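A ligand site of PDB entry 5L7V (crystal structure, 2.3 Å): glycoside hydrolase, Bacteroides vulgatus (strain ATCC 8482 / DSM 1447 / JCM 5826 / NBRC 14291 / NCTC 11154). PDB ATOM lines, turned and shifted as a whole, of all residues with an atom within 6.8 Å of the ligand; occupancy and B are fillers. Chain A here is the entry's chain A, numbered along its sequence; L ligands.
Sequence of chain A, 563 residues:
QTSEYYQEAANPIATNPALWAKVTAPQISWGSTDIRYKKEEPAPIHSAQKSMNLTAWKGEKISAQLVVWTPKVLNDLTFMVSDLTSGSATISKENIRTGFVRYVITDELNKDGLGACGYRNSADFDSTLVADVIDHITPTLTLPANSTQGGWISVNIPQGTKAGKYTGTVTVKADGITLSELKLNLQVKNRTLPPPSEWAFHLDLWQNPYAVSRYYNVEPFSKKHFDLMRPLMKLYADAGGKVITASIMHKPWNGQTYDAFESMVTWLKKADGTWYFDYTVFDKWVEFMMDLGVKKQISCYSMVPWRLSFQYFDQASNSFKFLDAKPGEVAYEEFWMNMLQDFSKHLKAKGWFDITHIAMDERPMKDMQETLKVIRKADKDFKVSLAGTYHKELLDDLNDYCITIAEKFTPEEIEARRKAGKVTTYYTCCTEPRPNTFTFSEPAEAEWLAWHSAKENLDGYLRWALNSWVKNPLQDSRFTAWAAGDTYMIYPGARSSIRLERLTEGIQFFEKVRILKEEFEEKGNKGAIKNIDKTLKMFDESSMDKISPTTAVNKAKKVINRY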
ATOM      1  N   ALA A 116     -31.018  12.897  10.226  1.00  0.00           N
ATOM      2  CA  ALA A 116     -29.688  13.133  10.785  1.00  0.00           C
ATOM      3  C   ALA A 116     -28.752  13.809   9.789  1.00  0.00           C
ATOM      4  O   ALA A 116     -27.555  13.591   9.821  1.00  0.00           O
ATOM      5  CB  ALA A 116     -29.104  11.825  11.243  1.00  0.00           C
ATOM      6  N   CYS A 117     -29.287  14.685   8.953  1.00  0.00           N
ATOM      7  CA  CYS A 117     -28.514  15.273   7.866  1.00  0.00           C
ATOM      8  C   CYS A 117     -27.986  16.609   8.356  1.00  0.00           C
ATOM      9  O   CYS A 117     -28.444  17.106   9.400  1.00  0.00           O
ATOM     10  CB  CYS A 117     -29.377  15.380   6.561  1.00  0.00           C
ATOM     11  SG  CYS A 117     -29.687  13.788   5.655  1.00  0.00           S
ATOM     12  N   TRP A 206     -18.565   1.506   0.493  1.00  0.00           N
ATOM     13  CA  TRP A 206     -17.455   2.164  -0.177  1.00  0.00           C
ATOM     14  C   TRP A 206     -16.232   2.239   0.727  1.00  0.00           C
ATOM     15  O   TRP A 206     -16.343   2.663   1.878  1.00  0.00           O
ATOM     16  CB  TRP A 206     -17.799   3.564  -0.633  1.00  0.00           C
ATOM     17  CG  TRP A 206     -18.975   3.664  -1.492  1.00  0.00           C
ATOM     18  CD1 TRP A 206     -19.584   2.641  -2.136  1.00  0.00           C
ATOM     19  CD2 TRP A 206     -19.665   4.841  -1.875  1.00  0.00           C
ATOM     20  NE1 TRP A 206     -20.665   3.087  -2.823  1.00  0.00           N
ATOM     21  CE2 TRP A 206     -20.725   4.444  -2.706  1.00  0.00           C
ATOM     22  CE3 TRP A 206     -19.520   6.195  -1.558  1.00  0.00           C
ATOM     23  CZ2 TRP A 206     -21.638   5.347  -3.252  1.00  0.00           C
ATOM     24  CZ3 TRP A 206     -20.422   7.114  -2.135  1.00  0.00           C
ATOM     25  CH2 TRP A 206     -21.464   6.671  -2.958  1.00  0.00           C
ATOM     26  N   TRP A 253     -15.582  13.394  -3.990  1.00  0.00           N
ATOM     27  CA  TRP A 253     -16.605  13.937  -3.103  1.00  0.00           C
ATOM     28  C   TRP A 253     -16.176  15.238  -2.441  1.00  0.00           C
ATOM     29  O   TRP A 253     -16.763  15.616  -1.461  1.00  0.00           O
ATOM     30  CB  TRP A 253     -16.947  12.886  -2.060  1.00  0.00           C
ATOM     31  CG  TRP A 253     -17.492  11.603  -2.638  1.00  0.00           C
ATOM     32  CD1 TRP A 253     -18.778  11.363  -2.988  1.00  0.00           C
ATOM     33  CD2 TRP A 253     -16.775  10.389  -2.888  1.00  0.00           C
ATOM     34  NE1 TRP A 253     -18.921  10.065  -3.443  1.00  0.00           N
ATOM     35  CE2 TRP A 253     -17.706   9.452  -3.410  1.00  0.00           C
ATOM     36  CE3 TRP A 253     -15.454   9.981  -2.692  1.00  0.00           C
ATOM     37  CZ2 TRP A 253     -17.347   8.158  -3.762  1.00  0.00           C
ATOM     38  CZ3 TRP A 253     -15.093   8.676  -3.030  1.00  0.00           C
ATOM     39  CH2 TRP A 253     -16.038   7.785  -3.569  1.00  0.00           C
ATOM     40  N   GLN A 256     -15.594  15.460   1.579  1.00  0.00           N
ATOM     41  CA  GLN A 256     -16.673  15.510   2.564  1.00  0.00           C
ATOM     42  C   GLN A 256     -16.291  14.680   3.804  1.00  0.00           C
ATOM     43  O   GLN A 256     -16.854  14.906   4.851  1.00  0.00           O
ATOM     44  CB  GLN A 256     -18.023  15.028   1.979  1.00  0.00           C
ATOM     45  CG  GLN A 256     -18.114  13.518   1.860  1.00  0.00           C
ATOM     46  CD  GLN A 256     -19.364  12.980   1.201  1.00  0.00           C
ATOM     47  OE1 GLN A 256     -20.478  13.547   1.322  1.00  0.00           O
ATOM     48  NE2 GLN A 256     -19.204  11.818   0.543  1.00  0.00           N
ATOM     49  N   TRP A 306     -18.338  16.203  -6.809  1.00  0.00           N
ATOM     50  CA  TRP A 306     -19.202  17.126  -6.126  1.00  0.00           C
ATOM     51  C   TRP A 306     -18.861  18.614  -6.343  1.00  0.00           C
ATOM     52  O   TRP A 306     -19.731  19.460  -6.256  1.00  0.00           O
ATOM     53  CB  TRP A 306     -19.283  16.716  -4.644  1.00  0.00           C
ATOM     54  CG  TRP A 306     -20.202  15.493  -4.454  1.00  0.00           C
ATOM     55  CD1 TRP A 306     -20.453  14.491  -5.374  1.00  0.00           C
ATOM     56  CD2 TRP A 306     -20.983  15.163  -3.289  1.00  0.00           C
ATOM     57  NE1 TRP A 306     -21.351  13.570  -4.847  1.00  0.00           N
ATOM     58  CE2 TRP A 306     -21.685  13.965  -3.577  1.00  0.00           C
ATOM     59  CE3 TRP A 306     -21.119  15.737  -2.022  1.00  0.00           C
ATOM     60  CZ2 TRP A 306     -22.520  13.348  -2.644  1.00  0.00           C
ATOM     61  CZ3 TRP A 306     -21.976  15.137  -1.104  1.00  0.00           C
ATOM     62  CH2 TRP A 306     -22.659  13.952  -1.419  1.00  0.00           C
ATOM     63  N   MET A 360     -21.436   7.519 -10.093  1.00  0.00           N
ATOM     64  CA  MET A 360     -21.897   8.859  -9.688  1.00  0.00           C
ATOM     65  C   MET A 360     -22.715   8.765  -8.444  1.00  0.00           C
ATOM     66  O   MET A 360     -23.379   7.769  -8.190  1.00  0.00           O
ATOM     67  CB  MET A 360     -22.754   9.521 -10.752  1.00  0.00           C
ATOM     68  CG  MET A 360     -22.448   8.973 -12.130  1.00  0.00           C
ATOM     69  SD  MET A 360     -20.830   9.508 -12.668  1.00  0.00           S
ATOM     70  CE  MET A 360     -21.310  10.500 -14.028  1.00  0.00           C
ATOM     71  N   ASP A 361     -22.696   9.854  -7.698  1.00  0.00           N
ATOM     72  CA  ASP A 361     -23.269   9.854  -6.379  1.00  0.00           C
ATOM     73  C   ASP A 361     -24.184  11.049  -6.309  1.00  0.00           C
ATOM     74  O   ASP A 361     -23.730  12.152  -6.132  1.00  0.00           O
ATOM     75  CB  ASP A 361     -22.111   9.893  -5.340  1.00  0.00           C
ATOM     76  CG  ASP A 361     -22.588   9.963  -3.904  1.00  0.00           C
ATOM     77  OD1 ASP A 361     -23.814   9.764  -3.645  1.00  0.00           O
ATOM     78  OD2 ASP A 361     -21.710  10.219  -3.036  1.00  0.00           O
ATOM     79  N   GLU A 362     -25.484  10.802  -6.436  1.00  0.00           N
ATOM     80  CA  GLU A 362     -26.535  11.777  -6.161  1.00  0.00           C
ATOM     81  C   GLU A 362     -26.505  13.038  -7.057  1.00  0.00           C
ATOM     82  O   GLU A 362     -26.667  14.161  -6.576  1.00  0.00           O
ATOM     83  CB  GLU A 362     -26.587  12.134  -4.678  1.00  0.00           C
ATOM     84  CG  GLU A 362     -27.052  11.010  -3.787  1.00  0.00           C
ATOM     85  CD  GLU A 362     -27.289  11.446  -2.337  1.00  0.00           C
ATOM     86  OE1 GLU A 362     -26.720  12.492  -1.937  1.00  0.00           O
ATOM     87  OE2 GLU A 362     -28.028  10.759  -1.580  1.00  0.00           O
ATOM     88  N   ALA A 387     -25.933   5.970  -7.555  1.00  0.00           N
ATOM     89  CA  ALA A 387     -26.605   5.883  -6.292  1.00  0.00           C
ATOM     90  C   ALA A 387     -27.237   7.235  -6.119  1.00  0.00           C
ATOM     91  O   ALA A 387     -26.541   8.231  -5.940  1.00  0.00           O
ATOM     92  CB  ALA A 387     -25.623   5.582  -5.182  1.00  0.00           C
ATOM     93  N   GLY A 388     -28.550   7.268  -6.208  1.00  0.00           N
ATOM     94  CA  GLY A 388     -29.276   8.537  -6.181  1.00  0.00           C
ATOM     95  C   GLY A 388     -30.771   8.425  -6.335  1.00  0.00           C
ATOM     96  O   GLY A 388     -31.382   7.508  -5.807  1.00  0.00           O
ATOM     97  N   CYS A 402     -28.875   2.346  -7.726  1.00  0.00           N
ATOM     98  CA  CYS A 402     -29.196   2.249  -6.333  1.00  0.00           C
ATOM     99  C   CYS A 402     -30.000   3.457  -5.898  1.00  0.00           C
ATOM    100  O   CYS A 402     -29.581   4.587  -6.055  1.00  0.00           O
ATOM    101  CB  CYS A 402     -27.903   2.172  -5.521  1.00  0.00           C
ATOM    102  SG  CYS A 402     -28.239   2.045  -3.750  1.00  0.00           S
ATOM    103  N   TYR A 427     -30.230   2.337  -0.790  1.00  0.00           N
ATOM    104  CA  TYR A 427     -29.421   2.856   0.285  1.00  0.00           C
ATOM    105  C   TYR A 427     -30.209   3.645   1.301  1.00  0.00           C
ATOM    106  O   TYR A 427     -31.332   4.051   1.071  1.00  0.00           O
ATOM    107  CB  TYR A 427     -28.253   3.681  -0.219  1.00  0.00           C
ATOM    108  CG  TYR A 427     -28.620   5.020  -0.788  1.00  0.00           C
ATOM    109  CD1 TYR A 427     -29.126   5.130  -2.090  1.00  0.00           C
ATOM    110  CD2 TYR A 427     -28.415   6.185  -0.076  1.00  0.00           C
ATOM    111  CE1 TYR A 427     -29.452   6.363  -2.638  1.00  0.00           C
ATOM    112  CE2 TYR A 427     -28.720   7.410  -0.624  1.00  0.00           C
ATOM    113  CZ  TYR A 427     -29.239   7.484  -1.901  1.00  0.00           C
ATOM    114  OH  TYR A 427     -29.541   8.688  -2.443  1.00  0.00           O
ATOM    115  N   THR A 428     -29.634   3.707   2.487  1.00  0.00           N
ATOM    116  CA  THR A 428     -29.946   4.731   3.440  1.00  0.00           C
ATOM    117  C   THR A 428     -28.639   5.510   3.571  1.00  0.00           C
ATOM    118  O   THR A 428     -27.505   5.042   3.222  1.00  0.00           O
ATOM    119  CB  THR A 428     -30.340   4.141   4.795  1.00  0.00           C
ATOM    120  OG1 THR A 428     -29.221   3.436   5.373  1.00  0.00           O
ATOM    121  CG2 THR A 428     -31.480   3.204   4.669  1.00  0.00           C
ATOM    122  N   CYS A 429     -28.831   6.707   4.079  1.00  0.00           N
ATOM    123  CA  CYS A 429     -27.800   7.713   4.282  1.00  0.00           C
ATOM    124  C   CYS A 429     -28.176   8.428   5.599  1.00  0.00           C
ATOM    125  O   CYS A 429     -28.799   7.836   6.489  1.00  0.00           O
ATOM    126  CB  CYS A 429     -27.838   8.656   3.061  1.00  0.00           C
ATOM    127  SG  CYS A 429     -29.413   9.520   2.830  1.00  0.00           S
ATOM    128  N   CYS A 430     -27.803   9.702   5.732  1.00  0.00           N
ATOM    129  CA  CYS A 430     -28.264  10.517   6.834  1.00  0.00           C
ATOM    130  C   CYS A 430     -29.779  10.831   6.902  1.00  0.00           C
ATOM    131  O   CYS A 430     -30.218  11.269   7.945  1.00  0.00           O
ATOM    132  CB  CYS A 430     -27.492  11.836   6.800  1.00  0.00           C
ATOM    133  SG  CYS A 430     -27.835  12.841   5.314  1.00  0.00           S
ATOM    134  N   THR A 431     -30.555  10.669   5.825  1.00  0.00           N
ATOM    135  CA  THR A 431     -31.989  11.143   5.832  1.00  0.00           C
ATOM    136  C   THR A 431     -32.869  10.408   6.847  1.00  0.00           C
ATOM    137  O   THR A 431     -33.766  11.002   7.444  1.00  0.00           O
ATOM    138  CB  THR A 431     -32.733  11.031   4.441  1.00  0.00           C
ATOM    139  OG1 THR A 431     -31.828  10.955   3.312  1.00  0.00           O
ATOM    140  CG2 THR A 431     -33.745  12.202   4.257  1.00  0.00           C
ATOM    141  N   PHE A 438     -26.089   4.249  12.359  1.00  0.00           N
ATOM    142  CA  PHE A 438     -25.408   5.167  13.258  1.00  0.00           C
ATOM    143  C   PHE A 438     -24.979   4.419  14.540  1.00  0.00           C
ATOM    144  O   PHE A 438     -25.599   3.414  14.898  1.00  0.00           O
ATOM    145  CB  PHE A 438     -26.341   6.298  13.631  1.00  0.00           C
ATOM    146  CG  PHE A 438     -27.013   6.950  12.471  1.00  0.00           C
ATOM    147  CD1 PHE A 438     -26.265   7.366  11.362  1.00  0.00           C
ATOM    148  CD2 PHE A 438     -28.377   7.149  12.469  1.00  0.00           C
ATOM    149  CE1 PHE A 438     -26.894   7.955  10.262  1.00  0.00           C
ATOM    150  CE2 PHE A 438     -28.998   7.736  11.374  1.00  0.00           C
ATOM    151  CZ  PHE A 438     -28.255   8.154  10.274  1.00  0.00           C
ATOM    152  N   LEU A 462     -26.528  -0.877  -0.308  1.00  0.00           N
ATOM    153  CA  LEU A 462     -25.405   0.032  -0.450  1.00  0.00           C
ATOM    154  C   LEU A 462     -25.328   1.016   0.715  1.00  0.00           C
ATOM    155  O   LEU A 462     -26.312   1.597   1.108  1.00  0.00           O
ATOM    156  CB  LEU A 462     -25.557   0.808  -1.742  1.00  0.00           C
ATOM    157  CG  LEU A 462     -24.383   1.722  -2.111  1.00  0.00           C
ATOM    158  CD1 LEU A 462     -24.229   1.801  -3.656  1.00  0.00           C
ATOM    159  CD2 LEU A 462     -24.483   3.125  -1.496  1.00  0.00           C
ATOM    160  N   ARG A 463     -24.120   1.214   1.217  1.00  0.00           N
ATOM    161  CA  ARG A 463     -23.827   2.318   2.115  1.00  0.00           C
ATOM    162  C   ARG A 463     -22.486   2.928   1.760  1.00  0.00           C
ATOM    163  O   ARG A 463     -21.564   2.259   1.307  1.00  0.00           O
ATOM    164  CB  ARG A 463     -23.825   1.848   3.549  1.00  0.00           C
ATOM    165  CG  ARG A 463     -24.118   2.991   4.486  1.00  0.00           C
ATOM    166  CD  ARG A 463     -24.489   2.576   5.909  1.00  0.00           C
ATOM    167  NE  ARG A 463     -25.411   3.565   6.478  1.00  0.00           N
ATOM    168  CZ  ARG A 463     -25.107   4.835   6.748  1.00  0.00           C
ATOM    169  NH1 ARG A 463     -26.026   5.642   7.243  1.00  0.00           N
ATOM    170  NH2 ARG A 463     -23.907   5.359   6.510  1.00  0.00           N
ATOM    171  N   TRP A 464     -22.409   4.215   1.976  1.00  0.00           N
ATOM    172  CA  TRP A 464     -21.399   5.044   1.377  1.00  0.00           C
ATOM    173  C   TRP A 464     -20.075   5.111   2.106  1.00  0.00           C
ATOM    174  O   TRP A 464     -19.154   5.754   1.627  1.00  0.00           O
ATOM    175  CB  TRP A 464     -21.943   6.458   1.228  1.00  0.00           C
ATOM    176  CG  TRP A 464     -21.938   7.188   2.513  1.00  0.00           C
ATOM    177  CD1 TRP A 464     -22.801   7.035   3.540  1.00  0.00           C
ATOM    178  CD2 TRP A 464     -20.995   8.168   2.916  1.00  0.00           C
ATOM    179  NE1 TRP A 464     -22.468   7.869   4.562  1.00  0.00           N
ATOM    180  CE2 TRP A 464     -21.361   8.585   4.210  1.00  0.00           C
ATOM    181  CE3 TRP A 464     -19.886   8.745   2.308  1.00  0.00           C
ATOM    182  CZ2 TRP A 464     -20.643   9.544   4.903  1.00  0.00           C
ATOM    183  CZ3 TRP A 464     -19.199   9.703   2.973  1.00  0.00           C
ATOM    184  CH2 TRP A 464     -19.571  10.101   4.268  1.00  0.00           C
ATOM    185  N   TRP A 482     -23.400  14.884  10.079  1.00  0.00           N
ATOM    186  CA  TRP A 482     -24.220  13.669  10.227  1.00  0.00           C
ATOM    187  C   TRP A 482     -24.222  13.093  11.613  1.00  0.00           C
ATOM    188  O   TRP A 482     -23.414  13.434  12.461  1.00  0.00           O
ATOM    189  CB  TRP A 482     -23.859  12.604   9.171  1.00  0.00           C
ATOM    190  CG  TRP A 482     -23.701  13.236   7.809  1.00  0.00           C
ATOM    191  CD1 TRP A 482     -24.649  13.977   7.142  1.00  0.00           C
ATOM    192  CD2 TRP A 482     -22.512  13.286   7.011  1.00  0.00           C
ATOM    193  NE1 TRP A 482     -24.126  14.473   5.989  1.00  0.00           N
ATOM    194  CE2 TRP A 482     -22.821  14.066   5.866  1.00  0.00           C
ATOM    195  CE3 TRP A 482     -21.240  12.753   7.127  1.00  0.00           C
ATOM    196  CZ2 TRP A 482     -21.877  14.330   4.858  1.00  0.00           C
ATOM    197  CZ3 TRP A 482     -20.293  13.027   6.118  1.00  0.00           C
ATOM    198  CH2 TRP A 482     -20.638  13.798   4.991  1.00  0.00           C
ATOM    199  N   ASP A 486     -22.022   7.517  10.909  1.00  0.00           N
ATOM    200  CA  ASP A 486     -22.400   7.581   9.489  1.00  0.00           C
ATOM    201  C   ASP A 486     -21.235   7.276   8.557  1.00  0.00           C
ATOM    202  O   ASP A 486     -21.418   6.686   7.482  1.00  0.00           O
ATOM    203  CB  ASP A 486     -22.920   8.957   9.118  1.00  0.00           C
ATOM    204  CG  ASP A 486     -23.647   8.998   7.772  1.00  0.00           C
ATOM    205  OD1 ASP A 486     -24.458   8.105   7.431  1.00  0.00           O
ATOM    206  OD2 ASP A 486     -23.462   9.988   7.049  1.00  0.00           O
HETATM  207  C1  LIG L   1     -25.361  10.338   0.731  1.00  0.00           C
HETATM  208  S1  LIG L   1     -25.551   8.592   0.726  1.00  0.00           S
HETATM  209  C2  LIG L   1     -24.203  10.526  -0.251  1.00  0.00           C
HETATM  210  N1  LIG L   1     -24.331   9.399  -1.195  1.00  0.00           N
HETATM  211  C3  LIG L   1     -22.826  10.405   0.419  1.00  0.00           C
HETATM  212  O1  LIG L   1     -21.805  11.011  -0.391  1.00  0.00           O
HETATM  213  C4  LIG L   1     -22.777  11.123   1.764  1.00  0.00           C
HETATM  214  O2  LIG L   1     -22.832  12.526   1.530  1.00  0.00           O
HETATM  215  C5  LIG L   1     -23.907  10.650   2.661  1.00  0.00           C
HETATM  216  O3  LIG L   1     -25.142  10.926   2.010  1.00  0.00           O
HETATM  217  C6  LIG L   1     -23.905  11.311   4.040  1.00  0.00           C
HETATM  218  O4  LIG L   1     -24.797  10.572   4.888  1.00  0.00           O
HETATM  219  C7  LIG L   1     -25.030   8.430  -0.829  1.00  0.00           C
HETATM  220  C8  LIG L   1     -25.384   7.293  -1.740  1.00  0.00           C
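OD1 of Asp 361 sits at hydrogen-bond distance from N1 of the ligand.
The side-chain amide oxygen (OE1) of Gln 256 is in hydrogen-bond range of an oxygen (O2) of the ligand.
OD2 of Asp 486 lies within hydrogen-bond range of O4 of the ligand.
An oxygen (O4) of the ligand sits at hydrogen-bond distance from the backbone NH of Cys 430.
Merely in contact with the ligand: Trp 306, Cys 429, Trp 482, Tyr 427, Glu 362, Trp 464 and Ala 387.
Hydrophobic or aromatic side chains within 4 Å of the ligand: Trp 306, Ala 387, Tyr 427, Trp 464 and Trp 482.
Within 4 Å of the ligand: Gln 256, Trp 306, Asp 361, Glu 362, Ala 387, Tyr 427, Cys 429, Cys 430, Trp 464, Trp 482 and Asp 486.
The nearest printed residue that does not touch the ligand is Trp 253 (4.004 Å).
O of Asp 361 lies within hydrogen-bond range of NE1 of Trp 306 (3.1 Å).
The indole nitrogen of Trp 464 is in hydrogen-bond range of the backbone carbonyl oxygen of Asp 486, 3.3 Å away.
SG of Cys 430 is disulfide-bonded to SG of Cys 117 (2.1 Å).
O of Cys 430 lies within hydrogen-bond range of N of Ala 116.
The side-chain sulfur (SG) of Cys 429 is in hydrogen-bond range of the side-chain hydroxyl (OG1) of Thr 431 (2.9 Å).
The side-chain sulfur (SG) of Cys 402 is in hydrogen-bond range of the backbone NH (N) of Tyr 427, 3.6 Å away.
The backbone NH of Glu 362 lies within hydrogen-bond range of the backbone carbonyl oxygen of Ala 387 (2.8 Å).
The backbone NH (N) of Ala 387 lies within hydrogen-bond range of the backbone carbonyl oxygen (O) of Met 360 (3.2 Å).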
